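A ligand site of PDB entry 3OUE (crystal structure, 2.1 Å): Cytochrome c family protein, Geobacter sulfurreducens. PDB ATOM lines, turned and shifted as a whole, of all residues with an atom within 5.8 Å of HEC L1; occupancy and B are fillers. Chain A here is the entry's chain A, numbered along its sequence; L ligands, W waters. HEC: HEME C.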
ATOM      1  N   PRO A   4     -28.633 -22.870  -2.493  1.00  0.00           N
ATOM      2  CA  PRO A   4     -27.929 -22.924  -1.209  1.00  0.00           C
ATOM      3  C   PRO A   4     -27.420 -21.508  -0.919  1.00  0.00           C
ATOM      4  O   PRO A   4     -27.024 -20.786  -1.839  1.00  0.00           O
ATOM      5  CB  PRO A   4     -26.804 -23.923  -1.476  1.00  0.00           C
ATOM      6  CG  PRO A   4     -26.581 -23.812  -2.974  1.00  0.00           C
ATOM      7  CD  PRO A   4     -27.994 -23.740  -3.495  1.00  0.00           C
ATOM      8  N   VAL A   7     -22.337 -19.412   3.082  1.00  0.00           N
ATOM      9  CA  VAL A   7     -22.009 -20.116   4.311  1.00  0.00           C
ATOM     10  C   VAL A   7     -21.070 -19.319   5.204  1.00  0.00           C
ATOM     11  O   VAL A   7     -20.088 -18.743   4.727  1.00  0.00           O
ATOM     12  CB  VAL A   7     -21.362 -21.465   4.000  1.00  0.00           C
ATOM     13  CG1 VAL A   7     -21.103 -22.235   5.298  1.00  0.00           C
ATOM     14  CG2 VAL A   7     -22.252 -22.253   3.062  1.00  0.00           C
ATOM     15  N   PHE A   9     -18.560 -19.489   8.527  1.00  0.00           N
ATOM     16  CA  PHE A   9     -17.815 -20.384   9.400  1.00  0.00           C
ATOM     17  C   PHE A   9     -17.435 -19.644  10.679  1.00  0.00           C
ATOM     18  O   PHE A   9     -16.595 -18.747  10.655  1.00  0.00           O
ATOM     19  CB  PHE A   9     -16.553 -20.886   8.698  1.00  0.00           C
ATOM     20  CG  PHE A   9     -16.828 -21.715   7.482  1.00  0.00           C
ATOM     21  CD1 PHE A   9     -17.237 -21.106   6.293  1.00  0.00           C
ATOM     22  CD2 PHE A   9     -16.698 -23.094   7.518  1.00  0.00           C
ATOM     23  CE1 PHE A   9     -17.518 -21.872   5.164  1.00  0.00           C
ATOM     24  CE2 PHE A   9     -16.972 -23.870   6.396  1.00  0.00           C
ATOM     25  CZ  PHE A   9     -17.379 -23.253   5.218  1.00  0.00           C
ATOM     26  N   PHE A  19     -18.183 -18.388   2.572  1.00  0.00           N
ATOM     27  CA  PHE A  19     -18.128 -19.114   1.302  1.00  0.00           C
ATOM     28  C   PHE A  19     -19.368 -18.711   0.523  1.00  0.00           C
ATOM     29  O   PHE A  19     -20.480 -18.754   1.046  1.00  0.00           O
ATOM     30  CB  PHE A  19     -18.152 -20.623   1.530  1.00  0.00           C
ATOM     31  CG  PHE A  19     -18.343 -21.406   0.257  1.00  0.00           C
ATOM     32  CD1 PHE A  19     -17.302 -21.549  -0.649  1.00  0.00           C
ATOM     33  CD2 PHE A  19     -19.568 -21.974  -0.038  1.00  0.00           C
ATOM     34  CE1 PHE A  19     -17.476 -22.240  -1.832  1.00  0.00           C
ATOM     35  CE2 PHE A  19     -19.763 -22.672  -1.222  1.00  0.00           C
ATOM     36  CZ  PHE A  19     -18.710 -22.812  -2.124  1.00  0.00           C
ATOM     37  N   HIS A  21     -21.914 -19.524  -2.338  1.00  0.00           N
ATOM     38  CA  HIS A  21     -22.384 -20.564  -3.241  1.00  0.00           C
ATOM     39  C   HIS A  21     -22.611 -19.941  -4.602  1.00  0.00           C
ATOM     40  O   HIS A  21     -22.168 -20.485  -5.613  1.00  0.00           O
ATOM     41  CB  HIS A  21     -23.699 -21.161  -2.733  1.00  0.00           C
ATOM     42  CG  HIS A  21     -23.538 -22.431  -1.959  1.00  0.00           C
ATOM     43  ND1 HIS A  21     -23.647 -22.520  -0.589  1.00  0.00           N
ATOM     44  CD2 HIS A  21     -23.259 -23.685  -2.389  1.00  0.00           C
ATOM     45  CE1 HIS A  21     -23.437 -23.798  -0.248  1.00  0.00           C
ATOM     46  NE2 HIS A  21     -23.200 -24.547  -1.306  1.00  0.00           N
ATOM     47  N   HIS A  24     -19.335 -19.511  -6.678  1.00  0.00           N
ATOM     48  CA  HIS A  24     -18.808 -20.781  -7.158  1.00  0.00           C
ATOM     49  C   HIS A  24     -19.753 -21.534  -8.100  1.00  0.00           C
ATOM     50  O   HIS A  24     -19.302 -22.332  -8.930  1.00  0.00           O
ATOM     51  CB  HIS A  24     -18.421 -21.663  -5.963  1.00  0.00           C
ATOM     52  CG  HIS A  24     -17.232 -21.143  -5.213  1.00  0.00           C
ATOM     53  ND1 HIS A  24     -17.269 -20.098  -4.329  1.00  0.00           N
ATOM     54  CD2 HIS A  24     -15.924 -21.526  -5.272  1.00  0.00           C
ATOM     55  CE1 HIS A  24     -16.015 -19.879  -3.883  1.00  0.00           C
ATOM     56  NE2 HIS A  24     -15.170 -20.730  -4.425  1.00  0.00           N
ATOM     57  N   LEU A  25     -21.054 -21.285  -7.980  1.00  0.00           N
ATOM     58  CA  LEU A  25     -22.006 -21.938  -8.853  1.00  0.00           C
ATOM     59  C   LEU A  25     -21.856 -21.413 -10.277  1.00  0.00           C
ATOM     60  O   LEU A  25     -22.378 -21.996 -11.232  1.00  0.00           O
ATOM     61  CB  LEU A  25     -23.438 -21.729  -8.356  1.00  0.00           C
ATOM     62  CG  LEU A  25     -23.826 -22.712  -7.232  1.00  0.00           C
ATOM     63  CD1 LEU A  25     -25.148 -22.322  -6.603  1.00  0.00           C
ATOM     64  CD2 LEU A  25     -23.902 -24.116  -7.834  1.00  0.00           C
ATOM     65  N   TYR A  28     -19.096 -24.174 -11.033  1.00  0.00           N
ATOM     66  CA  TYR A  28     -19.345 -25.585 -10.780  1.00  0.00           C
ATOM     67  C   TYR A  28     -20.786 -25.997 -10.561  1.00  0.00           C
ATOM     68  O   TYR A  28     -21.659 -25.180 -10.296  1.00  0.00           O
ATOM     69  CB  TYR A  28     -18.531 -26.053  -9.565  1.00  0.00           C
ATOM     70  CG  TYR A  28     -17.066 -25.690  -9.612  1.00  0.00           C
ATOM     71  CD1 TYR A  28     -16.574 -24.596  -8.880  1.00  0.00           C
ATOM     72  CD2 TYR A  28     -16.163 -26.429 -10.369  1.00  0.00           C
ATOM     73  CE1 TYR A  28     -15.226 -24.256  -8.919  1.00  0.00           C
ATOM     74  CE2 TYR A  28     -14.808 -26.107 -10.413  1.00  0.00           C
ATOM     75  CZ  TYR A  28     -14.349 -25.015  -9.678  1.00  0.00           C
ATOM     76  OH  TYR A  28     -13.005 -24.688  -9.716  1.00  0.00           O
ATOM     77  N   LYS A  29     -21.009 -27.304 -10.664  1.00  0.00           N
ATOM     78  CA  LYS A  29     -22.310 -27.921 -10.430  1.00  0.00           C
ATOM     79  C   LYS A  29     -22.165 -28.596  -9.069  1.00  0.00           C
ATOM     80  O   LYS A  29     -21.050 -28.895  -8.642  1.00  0.00           O
ATOM     81  CB  LYS A  29     -22.611 -28.944 -11.531  1.00  0.00           C
ATOM     82  CG  LYS A  29     -21.364 -29.638 -12.068  1.00  0.00           C
ATOM     83  CD  LYS A  29     -21.690 -30.742 -13.065  1.00  0.00           C
ATOM     84  CE  LYS A  29     -20.400 -31.412 -13.553  1.00  0.00           C
ATOM     85  NZ  LYS A  29     -20.614 -32.761 -14.140  1.00  0.00           N
ATOM     86  N   CYS A  30     -23.289 -28.827  -8.394  1.00  0.00           N
ATOM     87  CA  CYS A  30     -23.286 -29.426  -7.059  1.00  0.00           C
ATOM     88  C   CYS A  30     -22.333 -30.605  -6.809  1.00  0.00           C
ATOM     89  O   CYS A  30     -21.592 -30.576  -5.822  1.00  0.00           O
ATOM     90  CB  CYS A  30     -24.717 -29.844  -6.680  1.00  0.00           C
ATOM     91  SG  CYS A  30     -26.017 -28.625  -7.063  1.00  0.00           S
ATOM     92  N   ASN A  31     -22.355 -31.625  -7.663  1.00  0.00           N
ATOM     93  CA  ASN A  31     -21.506 -32.811  -7.444  1.00  0.00           C
ATOM     94  C   ASN A  31     -20.005 -32.610  -7.534  1.00  0.00           C
ATOM     95  O   ASN A  31     -19.229 -33.537  -7.277  1.00  0.00           O
ATOM     96  CB  ASN A  31     -21.913 -33.976  -8.366  1.00  0.00           C
ATOM     97  CG  ASN A  31     -21.612 -33.703  -9.829  1.00  0.00           C
ATOM     98  OD1 ASN A  31     -20.748 -32.902 -10.162  1.00  0.00           O
ATOM     99  ND2 ASN A  31     -22.313 -34.401 -10.723  1.00  0.00           N
ATOM    100  N   GLU A  32     -19.554 -31.415  -7.891  1.00  0.00           N
ATOM    101  CA  GLU A  32     -18.126 -31.213  -7.959  1.00  0.00           C
ATOM    102  C   GLU A  32     -17.555 -30.935  -6.581  1.00  0.00           C
ATOM    103  O   GLU A  32     -16.344 -30.948  -6.391  1.00  0.00           O
ATOM    104  CB  GLU A  32     -17.796 -30.100  -8.954  1.00  0.00           C
ATOM    105  CG  GLU A  32     -18.075 -30.550 -10.397  1.00  0.00           C
ATOM    106  CD  GLU A  32     -17.630 -29.537 -11.433  1.00  0.00           C
ATOM    107  OE1 GLU A  32     -18.420 -28.619 -11.762  1.00  0.00           O
ATOM    108  OE2 GLU A  32     -16.487 -29.679 -11.923  1.00  0.00           O
ATOM    109  N   CYS A  33     -18.440 -30.695  -5.615  1.00  0.00           N
ATOM    110  CA  CYS A  33     -18.022 -30.440  -4.234  1.00  0.00           C
ATOM    111  C   CYS A  33     -18.761 -31.328  -3.248  1.00  0.00           C
ATOM    112  O   CYS A  33     -18.242 -31.655  -2.182  1.00  0.00           O
ATOM    113  CB  CYS A  33     -18.298 -28.985  -3.852  1.00  0.00           C
ATOM    114  SG  CYS A  33     -17.393 -27.757  -4.816  1.00  0.00           S
ATOM    115  N   HIS A  34     -19.979 -31.690  -3.604  1.00  0.00           N
ATOM    116  CA  HIS A  34     -20.811 -32.530  -2.758  1.00  0.00           C
ATOM    117  C   HIS A  34     -20.907 -33.934  -3.349  1.00  0.00           C
ATOM    118  O   HIS A  34     -21.264 -34.081  -4.515  1.00  0.00           O
ATOM    119  CB  HIS A  34     -22.216 -31.923  -2.644  1.00  0.00           C
ATOM    120  CG  HIS A  34     -22.253 -30.637  -1.880  1.00  0.00           C
ATOM    121  ND1 HIS A  34     -22.080 -30.532  -0.522  1.00  0.00           N
ATOM    122  CD2 HIS A  34     -22.473 -29.370  -2.317  1.00  0.00           C
ATOM    123  CE1 HIS A  34     -22.202 -29.239  -0.183  1.00  0.00           C
ATOM    124  NE2 HIS A  34     -22.442 -28.495  -1.238  1.00  0.00           N
ATOM    125  N   LEU A  37     -16.019 -33.408  -1.250  1.00  0.00           N
ATOM    126  CA  LEU A  37     -15.361 -32.341  -0.520  1.00  0.00           C
ATOM    127  C   LEU A  37     -16.159 -31.885   0.703  1.00  0.00           C
ATOM    128  O   LEU A  37     -15.582 -31.673   1.762  1.00  0.00           O
ATOM    129  CB  LEU A  37     -15.088 -31.145  -1.448  1.00  0.00           C
ATOM    130  CG  LEU A  37     -14.153 -31.475  -2.623  1.00  0.00           C
ATOM    131  CD1 LEU A  37     -13.890 -30.222  -3.452  1.00  0.00           C
ATOM    132  CD2 LEU A  37     -12.855 -32.025  -2.073  1.00  0.00           C
ATOM    133  N   PHE A  38     -17.470 -31.754   0.550  1.00  0.00           N
ATOM    134  CA  PHE A  38     -18.313 -31.329   1.658  1.00  0.00           C
ATOM    135  C   PHE A  38     -19.624 -32.114   1.647  1.00  0.00           C
ATOM    136  O   PHE A  38     -20.091 -32.537   0.582  1.00  0.00           O
ATOM    137  CB  PHE A  38     -18.632 -29.828   1.566  1.00  0.00           C
ATOM    138  CG  PHE A  38     -17.428 -28.974   1.258  1.00  0.00           C
ATOM    139  CD1 PHE A  38     -17.042 -28.752  -0.062  1.00  0.00           C
ATOM    140  CD2 PHE A  38     -16.678 -28.413   2.281  1.00  0.00           C
ATOM    141  CE1 PHE A  38     -15.927 -27.977  -0.360  1.00  0.00           C
ATOM    142  CE2 PHE A  38     -15.545 -27.636   1.998  1.00  0.00           C
ATOM    143  CZ  PHE A  38     -15.172 -27.418   0.673  1.00  0.00           C
ATOM    144  N   ALA A  39     -20.204 -32.311   2.815  1.00  0.00           N
ATOM    145  CA  ALA A  39     -21.450 -33.042   2.934  1.00  0.00           C
ATOM    146  C   ALA A  39     -22.637 -32.107   2.780  1.00  0.00           C
ATOM    147  O   ALA A  39     -22.496 -30.880   2.824  1.00  0.00           O
ATOM    148  CB  ALA A  39     -21.518 -33.758   4.279  1.00  0.00           C
ATOM    149  N   TYR A  40     -23.817 -32.685   2.585  1.00  0.00           N
ATOM    150  CA  TYR A  40     -25.049 -31.913   2.447  1.00  0.00           C
ATOM    151  C   TYR A  40     -25.721 -31.769   3.813  1.00  0.00           C
ATOM    152  O   TYR A  40     -26.701 -31.035   3.953  1.00  0.00           O
ATOM    153  CB  TYR A  40     -26.023 -32.623   1.512  1.00  0.00           C
ATOM    154  CG  TYR A  40     -25.771 -32.454   0.039  1.00  0.00           C
ATOM    155  CD1 TYR A  40     -25.683 -31.189  -0.542  1.00  0.00           C
ATOM    156  CD2 TYR A  40     -25.676 -33.556  -0.800  1.00  0.00           C
ATOM    157  CE1 TYR A  40     -25.516 -31.032  -1.921  1.00  0.00           C
ATOM    158  CE2 TYR A  40     -25.519 -33.425  -2.177  1.00  0.00           C
ATOM    159  CZ  TYR A  40     -25.438 -32.148  -2.731  1.00  0.00           C
ATOM    160  OH  TYR A  40     -25.285 -32.022  -4.095  1.00  0.00           O
ATOM    161  N   LYS A  41     -25.193 -32.479   4.804  1.00  0.00           N
ATOM    162  CA  LYS A  41     -25.788 -32.442   6.147  1.00  0.00           C
ATOM    163  C   LYS A  41     -25.193 -31.402   7.091  1.00  0.00           C
ATOM    164  O   LYS A  41     -24.071 -30.940   6.904  1.00  0.00           O
ATOM    165  CB  LYS A  41     -25.704 -33.837   6.790  1.00  0.00           C
ATOM    166  CG  LYS A  41     -26.156 -33.878   8.246  1.00  0.00           C
ATOM    167  CD  LYS A  41     -26.742 -35.239   8.628  1.00  0.00           C
ATOM    168  CE  LYS A  41     -28.080 -35.477   7.931  1.00  0.00           C
ATOM    169  NZ  LYS A  41     -28.695 -36.782   8.309  1.00  0.00           N
ATOM    170  N   ALA A  42     -25.991 -31.055   8.104  1.00  0.00           N
ATOM    171  CA  ALA A  42     -25.589 -30.079   9.110  1.00  0.00           C
ATOM    172  C   ALA A  42     -24.498 -30.682   9.983  1.00  0.00           C
ATOM    173  O   ALA A  42     -24.089 -30.089  10.991  1.00  0.00           O
ATOM    174  CB  ALA A  42     -26.801 -29.698   9.964  1.00  0.00           C
ATOM    175  N   GLY A  43     -24.028 -31.869   9.604  1.00  0.00           N
ATOM    176  CA  GLY A  43     -22.984 -32.524  10.361  1.00  0.00           C
ATOM    177  C   GLY A  43     -21.649 -31.838  10.118  1.00  0.00           C
ATOM    178  O   GLY A  43     -21.173 -31.765   8.986  1.00  0.00           O
ATOM    179  N   LYS A  45     -17.522 -31.072  10.326  1.00  0.00           N
ATOM    180  CA  LYS A  45     -16.300 -31.815  10.018  1.00  0.00           C
ATOM    181  C   LYS A  45     -15.188 -30.781   9.979  1.00  0.00           C
ATOM    182  O   LYS A  45     -14.268 -30.863   9.168  1.00  0.00           O
ATOM    183  CB  LYS A  45     -16.406 -32.531   8.657  1.00  0.00           C
ATOM    184  CG  LYS A  45     -17.395 -33.709   8.624  1.00  0.00           C
ATOM    185  CD  LYS A  45     -17.212 -34.582   7.379  1.00  0.00           C
ATOM    186  CE  LYS A  45     -17.518 -33.831   6.089  1.00  0.00           C
ATOM    187  NZ  LYS A  45     -17.260 -34.648   4.860  1.00  0.00           N
HETATM  188 FE   HEC L   1     -22.827 -26.532  -1.298  1.00  0.00          FE
HETATM  189  CHA HEC L   1     -22.862 -26.283   2.141  1.00  0.00           C
HETATM  190  CHB HEC L   1     -26.088 -27.502  -1.285  1.00  0.00           C
HETATM  191  CHC HEC L   1     -22.809 -26.586  -4.754  1.00  0.00           C
HETATM  192  CHD HEC L   1     -19.439 -26.059  -1.297  1.00  0.00           C
HETATM  193  NA  HEC L   1     -24.159 -26.882   0.105  1.00  0.00           N
HETATM  194  C1A HEC L   1     -24.043 -26.670   1.478  1.00  0.00           C
HETATM  195  C2A HEC L   1     -25.304 -26.925   2.137  1.00  0.00           C
HETATM  196  C3A HEC L   1     -26.162 -27.361   1.198  1.00  0.00           C
HETATM  197  C4A HEC L   1     -25.462 -27.326  -0.064  1.00  0.00           C
HETATM  198  CMA HEC L   1     -27.603 -27.782   1.493  1.00  0.00           C
HETATM  199  CAA HEC L   1     -25.593 -26.783   3.625  1.00  0.00           C
HETATM  200  CBA HEC L   1     -25.677 -28.159   4.259  1.00  0.00           C
HETATM  201  CGA HEC L   1     -25.317 -28.148   5.731  1.00  0.00           C
HETATM  202  O1A HEC L   1     -24.143 -27.878   6.043  1.00  0.00           O
HETATM  203  O2A HEC L   1     -26.207 -28.426   6.571  1.00  0.00           O
HETATM  204  NB  HEC L   1     -24.160 -26.867  -2.693  1.00  0.00           N
HETATM  205  C1B HEC L   1     -25.479 -27.276  -2.520  1.00  0.00           C
HETATM  206  C2B HEC L   1     -26.159 -27.444  -3.804  1.00  0.00           C
HETATM  207  C3B HEC L   1     -25.244 -27.133  -4.774  1.00  0.00           C
HETATM  208  C4B HEC L   1     -24.017 -26.801  -4.093  1.00  0.00           C
HETATM  209  CMB HEC L   1     -27.622 -27.868  -4.019  1.00  0.00           C
HETATM  210  CAB HEC L   1     -25.480 -27.067  -6.285  1.00  0.00           C
HETATM  211  CBB HEC L   1     -26.547 -26.026  -6.627  1.00  0.00           C
HETATM  212  NC  HEC L   1     -21.459 -26.356  -2.702  1.00  0.00           N
HETATM  213  C1C HEC L   1     -21.599 -26.408  -4.092  1.00  0.00           C
HETATM  214  C2C HEC L   1     -20.322 -26.260  -4.780  1.00  0.00           C
HETATM  215  C3C HEC L   1     -19.382 -26.148  -3.789  1.00  0.00           C
HETATM  216  C4C HEC L   1     -20.086 -26.175  -2.524  1.00  0.00           C
HETATM  217  CMC HEC L   1     -20.123 -26.226  -6.309  1.00  0.00           C
HETATM  218  CAC HEC L   1     -17.850 -26.221  -3.921  1.00  0.00           C
HETATM  219  CBC HEC L   1     -17.264 -25.155  -4.841  1.00  0.00           C
HETATM  220  ND  HEC L   1     -21.464 -26.195   0.084  1.00  0.00           N
HETATM  221  C1D HEC L   1     -20.098 -26.024  -0.080  1.00  0.00           C
HETATM  222  C2D HEC L   1     -19.454 -25.684   1.171  1.00  0.00           C
HETATM  223  C3D HEC L   1     -20.399 -25.733   2.147  1.00  0.00           C
HETATM  224  C4D HEC L   1     -21.649 -26.069   1.488  1.00  0.00           C
HETATM  225  CMD HEC L   1     -18.002 -25.227   1.372  1.00  0.00           C
HETATM  226  CAD HEC L   1     -20.135 -25.485   3.632  1.00  0.00           C
HETATM  227  CBD HEC L   1     -19.906 -26.816   4.358  1.00  0.00           C
HETATM  228  CGD HEC L   1     -19.564 -26.623   5.823  1.00  0.00           C
HETATM  229  O1D HEC L   1     -20.307 -25.912   6.536  1.00  0.00           O
HETATM  230  O2D HEC L   1     -18.553 -27.207   6.270  1.00  0.00           O
HETATM  231 FE   HEC L   2     -13.182 -20.865  -3.989  1.00  0.00          FE
HETATM  232  CHA HEC L   2     -12.524 -18.114  -5.927  1.00  0.00           C
HETATM  233  CHB HEC L   2     -13.487 -18.806  -1.276  1.00  0.00           C
HETATM  234  CHC HEC L   2     -13.823 -23.608  -2.057  1.00  0.00           C
HETATM  235  CHD HEC L   2     -12.683 -22.908  -6.702  1.00  0.00           C
HETATM  236  NA  HEC L   2     -13.142 -18.895  -3.703  1.00  0.00           N
HETATM  237  C1A HEC L   2     -12.891 -17.887  -4.616  1.00  0.00           C
HETATM  238  C2A HEC L   2     -12.846 -16.568  -3.987  1.00  0.00           C
HETATM  239  C3A HEC L   2     -13.138 -16.782  -2.689  1.00  0.00           C
HETATM  240  C4A HEC L   2     -13.275 -18.212  -2.500  1.00  0.00           C
HETATM  241  CMA HEC L   2     -13.359 -15.720  -1.629  1.00  0.00           C
HETATM  242  CAA HEC L   2     -12.507 -15.216  -4.632  1.00  0.00           C
HETATM  243  CBA HEC L   2     -13.668 -14.768  -5.510  1.00  0.00           C
HETATM  244  CGA HEC L   2     -13.388 -13.477  -6.254  1.00  0.00           C
HETATM  245  O1A HEC L   2     -14.001 -12.435  -5.900  1.00  0.00           O
HETATM  246  O2A HEC L   2     -12.567 -13.485  -7.190  1.00  0.00           O
HETATM  247  NB  HEC L   2     -13.546 -21.149  -2.121  1.00  0.00           N
HETATM  248  C1B HEC L   2     -13.595 -20.179  -1.095  1.00  0.00           C
HETATM  249  C2B HEC L   2     -13.820 -20.793   0.188  1.00  0.00           C
HETATM  250  C3B HEC L   2     -13.877 -22.151  -0.030  1.00  0.00           C
HETATM  251  C4B HEC L   2     -13.767 -22.355  -1.451  1.00  0.00           C
HETATM  252  CMB HEC L   2     -14.004 -20.057   1.530  1.00  0.00           C
HETATM  253  CAB HEC L   2     -13.984 -23.255   1.030  1.00  0.00           C
HETATM  254  CBB HEC L   2     -15.187 -23.088   1.915  1.00  0.00           C
HETATM  255  NC  HEC L   2     -13.254 -22.818  -4.302  1.00  0.00           N
HETATM  256  C1C HEC L   2     -13.598 -23.812  -3.400  1.00  0.00           C
HETATM  257  C2C HEC L   2     -13.622 -25.125  -4.027  1.00  0.00           C
HETATM  258  C3C HEC L   2     -13.270 -24.933  -5.322  1.00  0.00           C
HETATM  259  C4C HEC L   2     -13.031 -23.504  -5.492  1.00  0.00           C
HETATM  260  CMC HEC L   2     -13.947 -26.457  -3.354  1.00  0.00           C
HETATM  261  CAC HEC L   2     -13.079 -26.007  -6.380  1.00  0.00           C
HETATM  262  CBC HEC L   2     -14.318 -26.869  -6.620  1.00  0.00           C
HETATM  263  ND  HEC L   2     -12.691 -20.591  -5.850  1.00  0.00           N
HETATM  264  C1D HEC L   2     -12.551 -21.543  -6.861  1.00  0.00           C
HETATM  265  C2D HEC L   2     -12.210 -20.917  -8.109  1.00  0.00           C
HETATM  266  C3D HEC L   2     -12.126 -19.585  -7.884  1.00  0.00           C
HETATM  267  C4D HEC L   2     -12.425 -19.386  -6.497  1.00  0.00           C
HETATM  268  CMD HEC L   2     -11.901 -21.573  -9.457  1.00  0.00           C
HETATM  269  CAD HEC L   2     -11.868 -18.541  -8.963  1.00  0.00           C
HETATM  270  CBD HEC L   2     -10.405 -18.251  -9.271  1.00  0.00           C
HETATM  271  CGD HEC L   2      -9.700 -17.513  -8.153  1.00  0.00           C
HETATM  272  O1D HEC L   2     -10.131 -16.396  -7.788  1.00  0.00           O
HETATM  273  O2D HEC L   2      -8.697 -18.051  -7.642  1.00  0.00           O
HETATM  274 FE   HEC L   3      -8.754 -19.449   7.090  1.00  0.00          FE
HETATM  275  CHA HEC L   3     -10.437 -21.444   9.313  1.00  0.00           C
HETATM  276  CHB HEC L   3      -6.706 -18.299   9.573  1.00  0.00           C
HETATM  277  CHC HEC L   3      -6.700 -17.921   4.737  1.00  0.00           C
HETATM  278  CHD HEC L   3     -10.958 -20.292   4.643  1.00  0.00           C
HETATM  279  NA  HEC L   3      -8.599 -19.809   9.008  1.00  0.00           N
HETATM  280  C1A HEC L   3      -9.294 -20.757   9.747  1.00  0.00           C
HETATM  281  C2A HEC L   3      -8.772 -20.841  11.101  1.00  0.00           C
HETATM  282  C3A HEC L   3      -7.780 -19.916  11.219  1.00  0.00           C
HETATM  283  C4A HEC L   3      -7.698 -19.240   9.919  1.00  0.00           C
HETATM  284  CMA HEC L   3      -6.900 -19.693  12.448  1.00  0.00           C
HETATM  285  CAA HEC L   3      -9.199 -21.844  12.163  1.00  0.00           C
HETATM  286  CBA HEC L   3      -8.581 -23.211  11.963  1.00  0.00           C
HETATM  287  CGA HEC L   3      -7.070 -23.182  12.039  1.00  0.00           C
HETATM  288  O1A HEC L   3      -6.539 -22.652  13.041  1.00  0.00           O
HETATM  289  O2A HEC L   3      -6.413 -23.675  11.088  1.00  0.00           O
HETATM  290  NB  HEC L   3      -7.090 -18.349   7.145  1.00  0.00           N
HETATM  291  C1B HEC L   3      -6.419 -17.886   8.263  1.00  0.00           C
HETATM  292  C2B HEC L   3      -5.235 -17.107   7.878  1.00  0.00           C
HETATM  293  C3B HEC L   3      -5.174 -17.105   6.522  1.00  0.00           C
HETATM  294  C4B HEC L   3      -6.330 -17.849   6.078  1.00  0.00           C
HETATM  295  CMB HEC L   3      -4.239 -16.435   8.822  1.00  0.00           C
HETATM  296  CAB HEC L   3      -4.118 -16.471   5.607  1.00  0.00           C
HETATM  297  CBB HEC L   3      -2.662 -16.700   5.994  1.00  0.00           C
HETATM  298  NC  HEC L   3      -8.807 -19.146   5.152  1.00  0.00           N
HETATM  299  C1C HEC L   3      -7.880 -18.502   4.309  1.00  0.00           C
HETATM  300  C2C HEC L   3      -8.277 -18.538   2.918  1.00  0.00           C
HETATM  301  C3C HEC L   3      -9.514 -19.162   2.899  1.00  0.00           C
HETATM  302  C4C HEC L   3      -9.823 -19.569   4.276  1.00  0.00           C
HETATM  303  CMC HEC L   3      -7.457 -18.040   1.734  1.00  0.00           C
HETATM  304  CAC HEC L   3     -10.462 -19.279   1.712  1.00  0.00           C
HETATM  305  CBC HEC L   3      -9.871 -20.031   0.534  1.00  0.00           C
HETATM  306  ND  HEC L   3     -10.420 -20.527   7.027  1.00  0.00           N
HETATM  307  C1D HEC L   3     -11.243 -20.731   5.927  1.00  0.00           C
HETATM  308  C2D HEC L   3     -12.410 -21.548   6.311  1.00  0.00           C
HETATM  309  C3D HEC L   3     -12.236 -21.889   7.614  1.00  0.00           C
HETATM  310  C4D HEC L   3     -10.996 -21.277   8.050  1.00  0.00           C
HETATM  311  CMD HEC L   3     -13.621 -21.908   5.465  1.00  0.00           C
HETATM  312  CAD HEC L   3     -13.124 -22.809   8.433  1.00  0.00           C
HETATM  313  CBD HEC L   3     -12.987 -24.247   7.963  1.00  0.00           C
HETATM  314  CGD HEC L   3     -13.890 -25.188   8.721  1.00  0.00           C
HETATM  315  O1D HEC L   3     -13.970 -26.376   8.331  1.00  0.00           O
HETATM  316  O2D HEC L   3     -14.527 -24.762   9.700  1.00  0.00           O
HETATM  317  O   HOH W   1     -20.184 -23.843   9.063  1.00  0.00           O
HETATM  318  O   HOH W   2     -21.589 -29.268   4.521  1.00  0.00           O
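O1A of HEC L1 sits close to O of Lys 41, at 3.2 Å. Merely in contact with HEC L1: Pro 4 (3.7 Å), Val 7 (3.8 Å), Phe 9 (3.7 Å), Phe 19 (3.4 Å), His 24 (3.8 Å), Leu 25 (3.5 Å), Tyr 28 (3.6 Å), Lys 29 (3.7 Å), Phe 38 (3.5 Å) and Tyr 40 (3.1 Å). Within 4 Å of HEC L1: Pro 4, Val 7, Phe 9, Phe 19, His 21, His 24, Leu 25, Tyr 28, Lys 29, Cys 30, Cys 33, His 34, Phe 38, Tyr 40, Lys 41 and Ala 42. The nearest printed residue that does not touch HEC L1 is Ala 39 (4.4 Å).
The side-chain sulfur (SG) of Cys 30 is covalently linked to a carbon (CAB) of HEC L1, 1.8 Å away. The side-chain sulfur (SG) of Cys 33 is covalently linked to a carbon (CAC) of HEC L1. A ring nitrogen (NE2) of His 34 is bound to an iron atom (FE) of HEC L1 (2.0 Å). NE2 of His 21 is bound to FE of HEC L1 (2.0 Å). An oxygen (O2A) of HEC L1 lies within hydrogen-bond range of the backbone NH of Ala 42, at 3.1 Å. A ring nitrogen (NE2) of His 24 binds an iron atom (FE) of HEC L2 (2.0 Å).
Water W2 bridges O of Ala 39 (2.5 Å) and O1A of HEC L1 (3.3 Å).
The backbone NH (N) of Phe 38 lies within hydrogen-bond range of the backbone carbonyl oxygen (O) of Cys 33, at 2.8 Å. A ring nitrogen (ND1) of His 34 lies within hydrogen-bond range of the backbone carbonyl oxygen of Phe 38, at 3.0 Å. A ring nitrogen (ND1) of His 34 is in hydrogen-bond range of the backbone carbonyl oxygen (O) of Ala 39 (3.4 Å). O of Phe 19 lies within hydrogen-bond range of N of Val 7 (2.8 Å). OE1 of Glu 32 lies within hydrogen-bond range of N of Lys 29 (3.1 Å).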
